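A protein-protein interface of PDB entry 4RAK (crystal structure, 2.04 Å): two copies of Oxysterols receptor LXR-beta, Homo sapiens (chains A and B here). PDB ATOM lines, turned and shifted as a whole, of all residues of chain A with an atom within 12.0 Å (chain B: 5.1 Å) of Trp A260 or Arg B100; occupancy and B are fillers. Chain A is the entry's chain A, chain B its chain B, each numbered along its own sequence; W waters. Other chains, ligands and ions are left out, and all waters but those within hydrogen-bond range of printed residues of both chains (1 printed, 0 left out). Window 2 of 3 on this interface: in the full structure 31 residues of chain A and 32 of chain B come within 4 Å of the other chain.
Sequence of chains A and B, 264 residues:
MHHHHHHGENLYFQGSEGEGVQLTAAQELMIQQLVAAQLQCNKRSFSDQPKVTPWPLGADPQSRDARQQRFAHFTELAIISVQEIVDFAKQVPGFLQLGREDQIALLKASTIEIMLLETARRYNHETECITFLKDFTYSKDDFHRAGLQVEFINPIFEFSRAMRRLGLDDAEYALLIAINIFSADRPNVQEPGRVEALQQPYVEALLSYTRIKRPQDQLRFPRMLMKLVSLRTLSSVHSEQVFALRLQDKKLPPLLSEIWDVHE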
ATOM      1  N   LYS A 251      25.898  14.630  17.857  1.00  0.00           N
ATOM      2  CA  LYS A 251      26.797  15.316  16.930  1.00  0.00           C
ATOM      3  C   LYS A 251      26.164  15.534  15.545  1.00  0.00           C
ATOM      4  O   LYS A 251      25.158  14.905  15.210  1.00  0.00           O
ATOM      5  CB  LYS A 251      28.125  14.555  16.796  1.00  0.00           C
ATOM      6  CG  LYS A 251      29.359  15.441  16.946  1.00  0.00           C
ATOM      7  CD  LYS A 251      29.998  15.804  15.609  1.00  0.00           C
ATOM      8  CE  LYS A 251      31.176  16.740  15.772  1.00  0.00           C
ATOM      9  NZ  LYS A 251      32.389  16.031  16.265  1.00  0.00           N
ATOM     10  N   LEU A 252      26.764  16.436  14.754  1.00  0.00           N
ATOM     11  CA  LEU A 252      26.304  16.796  13.412  1.00  0.00           C
ATOM     12  C   LEU A 252      26.297  15.596  12.453  1.00  0.00           C
ATOM     13  O   LEU A 252      27.326  14.934  12.306  1.00  0.00           O
ATOM     14  CB  LEU A 252      27.179  17.918  12.821  1.00  0.00           C
ATOM     15  CG  LEU A 252      27.050  19.306  13.447  1.00  0.00           C
ATOM     16  CD1 LEU A 252      28.294  20.136  13.167  1.00  0.00           C
ATOM     17  CD2 LEU A 252      25.800  20.023  12.953  1.00  0.00           C
ATOM     18  N   PRO A 253      25.148  15.317  11.786  1.00  0.00           N
ATOM     19  CA  PRO A 253      25.119  14.214  10.811  1.00  0.00           C
ATOM     20  C   PRO A 253      26.001  14.522   9.587  1.00  0.00           C
ATOM     21  O   PRO A 253      25.758  15.524   8.909  1.00  0.00           O
ATOM     22  CB  PRO A 253      23.631  14.085  10.456  1.00  0.00           C
ATOM     23  CG  PRO A 253      23.029  15.389  10.784  1.00  0.00           C
ATOM     24  CD  PRO A 253      23.832  15.982  11.900  1.00  0.00           C
ATOM     25  N   PRO A 254      27.054  13.698   9.335  1.00  0.00           N
ATOM     26  CA  PRO A 254      28.021  14.012   8.271  1.00  0.00           C
ATOM     27  C   PRO A 254      27.474  14.131   6.852  1.00  0.00           C
ATOM     28  O   PRO A 254      27.879  15.047   6.137  1.00  0.00           O
ATOM     29  CB  PRO A 254      29.040  12.870   8.366  1.00  0.00           C
ATOM     30  CG  PRO A 254      28.342  11.786   9.110  1.00  0.00           C
ATOM     31  CD  PRO A 254      27.465  12.495  10.083  1.00  0.00           C
ATOM     32  N   LEU A 255      26.582  13.221   6.436  1.00  0.00           N
ATOM     33  CA  LEU A 255      26.005  13.257   5.085  1.00  0.00           C
ATOM     34  C   LEU A 255      25.082  14.459   4.849  1.00  0.00           C
ATOM     35  O   LEU A 255      25.194  15.114   3.812  1.00  0.00           O
ATOM     36  CB  LEU A 255      25.295  11.942   4.758  1.00  0.00           C
ATOM     37  CG  LEU A 255      26.222  10.788   4.393  1.00  0.00           C
ATOM     38  CD1 LEU A 255      25.980   9.583   5.281  1.00  0.00           C
ATOM     39  CD2 LEU A 255      26.091  10.435   2.917  1.00  0.00           C
ATOM     40  N   LEU A 256      24.195  14.762   5.818  1.00  0.00           N
ATOM     41  CA  LEU A 256      23.292  15.923   5.746  1.00  0.00           C
ATOM     42  C   LEU A 256      24.109  17.229   5.768  1.00  0.00           C
ATOM     43  O   LEU A 256      23.755  18.170   5.067  1.00  0.00           O
ATOM     44  CB  LEU A 256      22.230  15.893   6.869  1.00  0.00           C
ATOM     45  CG  LEU A 256      21.051  16.885   6.778  1.00  0.00           C
ATOM     46  CD1 LEU A 256      20.052  16.479   5.709  1.00  0.00           C
ATOM     47  CD2 LEU A 256      20.352  17.007   8.118  1.00  0.00           C
ATOM     48  N   SER A 257      25.229  17.256   6.521  1.00  0.00           N
ATOM     49  CA  SER A 257      26.145  18.407   6.552  1.00  0.00           C
ATOM     50  C   SER A 257      26.777  18.614   5.171  1.00  0.00           C
ATOM     51  O   SER A 257      26.984  19.756   4.765  1.00  0.00           O
ATOM     52  CB  SER A 257      27.254  18.210   7.590  1.00  0.00           C
ATOM     53  OG  SER A 257      26.753  18.084   8.909  1.00  0.00           O
ATOM     54  N   GLU A 258      27.059  17.510   4.449  1.00  0.00           N
ATOM     55  CA  GLU A 258      27.677  17.565   3.122  1.00  0.00           C
ATOM     56  C   GLU A 258      26.766  18.175   2.067  1.00  0.00           C
ATOM     57  O   GLU A 258      27.252  18.860   1.170  1.00  0.00           O
ATOM     58  CB  GLU A 258      28.207  16.190   2.678  1.00  0.00           C
ATOM     59  CG  GLU A 258      29.511  15.776   3.353  1.00  0.00           C
ATOM     60  CD  GLU A 258      30.538  16.883   3.531  1.00  0.00           C
ATOM     61  OE1 GLU A 258      31.035  17.414   2.514  1.00  0.00           O
ATOM     62  OE2 GLU A 258      30.835  17.235   4.695  1.00  0.00           O
ATOM     63  N   ILE A 259      25.450  17.957   2.191  1.00  0.00           N
ATOM     64  CA  ILE A 259      24.449  18.551   1.296  1.00  0.00           C
ATOM     65  C   ILE A 259      24.241  20.044   1.679  1.00  0.00           C
ATOM     66  O   ILE A 259      23.905  20.857   0.821  1.00  0.00           O
ATOM     67  CB  ILE A 259      23.153  17.676   1.267  1.00  0.00           C
ATOM     68  CG1 ILE A 259      23.489  16.265   0.726  1.00  0.00           C
ATOM     69  CG2 ILE A 259      22.032  18.327   0.446  1.00  0.00           C
ATOM     70  CD1 ILE A 259      22.359  15.265   0.690  1.00  0.00           C
ATOM     71  N   TRP A 260      24.532  20.384   2.955  1.00  0.00           N
ATOM     72  CA  TRP A 260      24.451  21.712   3.600  1.00  0.00           C
ATOM     73  C   TRP A 260      23.036  22.113   3.962  1.00  0.00           C
ATOM     74  O   TRP A 260      22.799  22.486   5.106  1.00  0.00           O
ATOM     75  CB  TRP A 260      25.142  22.833   2.806  1.00  0.00           C
ATOM     76  CG  TRP A 260      26.609  22.651   2.639  1.00  0.00           C
ATOM     77  CD1 TRP A 260      27.275  22.429   1.470  1.00  0.00           C
ATOM     78  CD2 TRP A 260      27.606  22.681   3.673  1.00  0.00           C
ATOM     79  NE1 TRP A 260      28.624  22.315   1.709  1.00  0.00           N
ATOM     80  CE2 TRP A 260      28.854  22.460   3.054  1.00  0.00           C
ATOM     81  CE3 TRP A 260      27.563  22.862   5.068  1.00  0.00           C
ATOM     82  CZ2 TRP A 260      30.054  22.418   3.781  1.00  0.00           C
ATOM     83  CZ3 TRP A 260      28.751  22.813   5.787  1.00  0.00           C
ATOM     84  CH2 TRP A 260      29.978  22.599   5.143  1.00  0.00           C
ATOM     85  N   VAL B  86      16.324  20.568   1.544  1.00  0.00           N
ATOM     86  CA  VAL B  86      17.549  21.333   1.854  1.00  0.00           C
ATOM     87  C   VAL B  86      17.563  22.611   1.002  1.00  0.00           C
ATOM     88  O   VAL B  86      17.689  23.696   1.556  1.00  0.00           O
ATOM     89  CB  VAL B  86      18.850  20.505   1.689  1.00  0.00           C
ATOM     90  CG1 VAL B  86      20.086  21.391   1.840  1.00  0.00           C
ATOM     91  CG2 VAL B  86      18.905  19.374   2.700  1.00  0.00           C
ATOM     92  N   LYS B  90      16.928  26.610   2.354  1.00  0.00           N
ATOM     93  CA  LYS B  90      17.966  27.604   2.070  1.00  0.00           C
ATOM     94  C   LYS B  90      17.371  28.903   1.528  1.00  0.00           C
ATOM     95  O   LYS B  90      17.847  29.989   1.856  1.00  0.00           O
ATOM     96  CB  LYS B  90      19.015  27.034   1.119  1.00  0.00           C
ATOM     97  CG  LYS B  90      20.063  26.224   1.860  1.00  0.00           C
ATOM     98  CD  LYS B  90      20.990  25.535   0.868  1.00  0.00           C
ATOM     99  CE  LYS B  90      22.097  24.778   1.563  1.00  0.00           C
ATOM    100  NZ  LYS B  90      23.016  24.185   0.557  1.00  0.00           N
ATOM    101  N   LEU B  96      18.963  31.133   6.530  1.00  0.00           N
ATOM    102  CA  LEU B  96      20.420  31.339   6.383  1.00  0.00           C
ATOM    103  C   LEU B  96      21.058  32.255   7.440  1.00  0.00           C
ATOM    104  O   LEU B  96      22.283  32.289   7.514  1.00  0.00           O
ATOM    105  CB  LEU B  96      20.792  31.786   4.968  1.00  0.00           C
ATOM    106  CG  LEU B  96      20.792  30.651   3.940  1.00  0.00           C
ATOM    107  CD1 LEU B  96      21.081  31.157   2.548  1.00  0.00           C
ATOM    108  CD2 LEU B  96      21.798  29.572   4.320  1.00  0.00           C
ATOM    109  N   LEU B  98      20.606  31.759  10.730  1.00  0.00           N
ATOM    110  CA  LEU B  98      20.850  30.928  11.917  1.00  0.00           C
ATOM    111  C   LEU B  98      22.238  30.296  11.799  1.00  0.00           C
ATOM    112  O   LEU B  98      22.762  30.178  10.696  1.00  0.00           O
ATOM    113  CB  LEU B  98      19.820  29.817  12.016  1.00  0.00           C
ATOM    114  CG  LEU B  98      18.423  30.157  12.520  1.00  0.00           C
ATOM    115  CD1 LEU B  98      17.430  29.108  12.041  1.00  0.00           C
ATOM    116  CD2 LEU B  98      18.382  30.243  14.037  1.00  0.00           C
ATOM    117  N   GLY B  99      22.798  29.844  12.918  1.00  0.00           N
ATOM    118  CA  GLY B  99      24.048  29.091  12.906  1.00  0.00           C
ATOM    119  C   GLY B  99      23.966  27.838  12.042  1.00  0.00           C
ATOM    120  O   GLY B  99      22.882  27.272  11.881  1.00  0.00           O
ATOM    121  N   ARG B 100      25.110  27.403  11.482  1.00  0.00           N
ATOM    122  CA  ARG B 100      25.190  26.216  10.599  1.00  0.00           C
ATOM    123  C   ARG B 100      24.734  24.926  11.310  1.00  0.00           C
ATOM    124  O   ARG B 100      24.043  24.122  10.707  1.00  0.00           O
ATOM    125  CB  ARG B 100      26.611  26.055  10.015  1.00  0.00           C
ATOM    126  CG  ARG B 100      26.673  25.410   8.632  1.00  0.00           C
ATOM    127  CD  ARG B 100      26.263  26.378   7.532  1.00  0.00           C
ATOM    128  NE  ARG B 100      26.659  25.917   6.202  1.00  0.00           N
ATOM    129  CZ  ARG B 100      26.278  26.488   5.064  1.00  0.00           C
ATOM    130  NH1 ARG B 100      25.479  27.548   5.080  1.00  0.00           N
ATOM    131  NH2 ARG B 100      26.690  26.002   3.901  1.00  0.00           N
ATOM    132  N   GLU B 101      25.107  24.770  12.589  1.00  0.00           N
ATOM    133  CA  GLU B 101      24.758  23.627  13.434  1.00  0.00           C
ATOM    134  C   GLU B 101      23.237  23.528  13.659  1.00  0.00           C
ATOM    135  O   GLU B 101      22.666  22.435  13.554  1.00  0.00           O
ATOM    136  CB  GLU B 101      25.505  23.691  14.783  1.00  0.00           C
ATOM    137  CG  GLU B 101      27.012  23.459  14.655  1.00  0.00           C
ATOM    138  CD  GLU B 101      27.725  23.083  15.947  1.00  0.00           C
ATOM    139  OE1 GLU B 101      28.006  21.879  16.151  1.00  0.00           O
ATOM    140  OE2 GLU B 101      28.027  23.993  16.750  1.00  0.00           O
ATOM    141  N   ASP B 102      22.594  24.681  13.940  1.00  0.00           N
ATOM    142  CA  ASP B 102      21.152  24.776  14.157  1.00  0.00           C
ATOM    143  C   ASP B 102      20.391  24.536  12.856  1.00  0.00           C
ATOM    144  O   ASP B 102      19.341  23.910  12.873  1.00  0.00           O
ATOM    145  CB  ASP B 102      20.778  26.125  14.802  1.00  0.00           C
ATOM    146  CG  ASP B 102      20.989  26.167  16.297  1.00  0.00           C
ATOM    147  OD1 ASP B 102      21.401  25.136  16.870  1.00  0.00           O
ATOM    148  OD2 ASP B 102      20.707  27.229  16.914  1.00  0.00           O
ATOM    149  N   GLN B 103      20.933  24.995  11.735  1.00  0.00           N
ATOM    150  CA  GLN B 103      20.338  24.798  10.412  1.00  0.00           C
ATOM    151  C   GLN B 103      20.146  23.299  10.104  1.00  0.00           C
ATOM    152  O   GLN B 103      19.087  22.892   9.661  1.00  0.00           O
ATOM    153  CB  GLN B 103      21.202  25.456   9.329  1.00  0.00           C
ATOM    154  CG  GLN B 103      21.047  26.976   9.259  1.00  0.00           C
ATOM    155  CD  GLN B 103      21.841  27.627   8.153  1.00  0.00           C
ATOM    156  OE1 GLN B 103      22.408  28.711   8.347  1.00  0.00           O
ATOM    157  NE2 GLN B 103      21.805  27.047   6.941  1.00  0.00           N
ATOM    158  N   ILE B 104      21.207  22.510  10.333  1.00  0.00           N
ATOM    159  CA  ILE B 104      21.287  21.075  10.099  1.00  0.00           C
ATOM    160  C   ILE B 104      20.383  20.352  11.095  1.00  0.00           C
ATOM    161  O   ILE B 104      19.635  19.457  10.693  1.00  0.00           O
ATOM    162  CB  ILE B 104      22.773  20.610  10.164  1.00  0.00           C
ATOM    163  CG1 ILE B 104      23.605  21.263   9.033  1.00  0.00           C
ATOM    164  CG2 ILE B 104      22.892  19.086  10.125  1.00  0.00           C
ATOM    165  CD1 ILE B 104      25.130  21.229   9.236  1.00  0.00           C
ATOM    166  N   LEU B 107      16.765  20.878  10.041  1.00  0.00           N
ATOM    167  CA  LEU B 107      16.528  20.067   8.868  1.00  0.00           C
ATOM    168  C   LEU B 107      16.519  18.562   9.173  1.00  0.00           C
ATOM    169  O   LEU B 107      15.804  17.806   8.510  1.00  0.00           O
ATOM    170  CB  LEU B 107      17.549  20.395   7.782  1.00  0.00           C
ATOM    171  CG  LEU B 107      17.257  21.629   6.911  1.00  0.00           C
ATOM    172  CD1 LEU B 107      17.974  21.516   5.607  1.00  0.00           C
ATOM    173  CD2 LEU B 107      15.785  21.794   6.589  1.00  0.00           C
HETATM  174  O   HOH W   1      22.210  25.094   4.977  1.00  0.00           O
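NZ of Lys B90 sits at hydrogen-bond distance from O of Ile A259, at 3.5 Å.
The side-chain hydroxyl (OG) of Ser A257 sits at hydrogen-bond distance from the backbone carbonyl oxygen (O) of Pro A253 (2.7 Å).
Among the printed residues, merely in contact across the chains: Leu A252 with Glu B101, Leu A252 with Ile B104, Pro A253 with Ile B104, Leu A256 with Ile B104, Ser A257 with Ile B104, Ile A259 with Val B86, Trp A260 with Val B86, Trp A260 with Lys B90 and Trp A260 with Arg B100.
Printed residues of chain B within 4 Å of Pro A253: Ile B104 (3.7 Å).
Printed residues of chain B within 4 Å of Leu A256: Ile B104 (3.6 Å).
No residue of chain A comes within 4 Å of Leu B98.
Of chain A, only Trp A260 comes within 4 Å of Arg B100.
Of chain A, only Leu A252 comes within 4 Å of Glu B101.
No residue of chain A comes within 4 Å of Gln B103.
Of chain A, only Leu A252, Pro A253, Leu A256 and Ser A257 come within 4 Å of Ile B104.
The nearest residue of chain A that does not touch Arg B100 is Leu A252 (5.0 Å).
The nearest printed residue of chain B that does not touch Ser A257 is Arg B100 (6.3 Å).
Hydrophobic or aromatic side chains of chain B within 4 Å of the printed part of chain A: Val B86 and Ile B104.
Among the printed residues, no Asp or Glu carboxylate lies within 4 Å of a Lys or Arg side-chain nitrogen of the other chain.
No position is printed for both chains.
Of the 10 pairs that touch across the chains among the printed residues, none has its exchanged pair printed and touching as well.
Water W1 bridges the backbone carbonyl oxygen of Trp A260 (2.7 Å) and the side-chain amide nitrogen of Gln B103 (2.8 Å).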
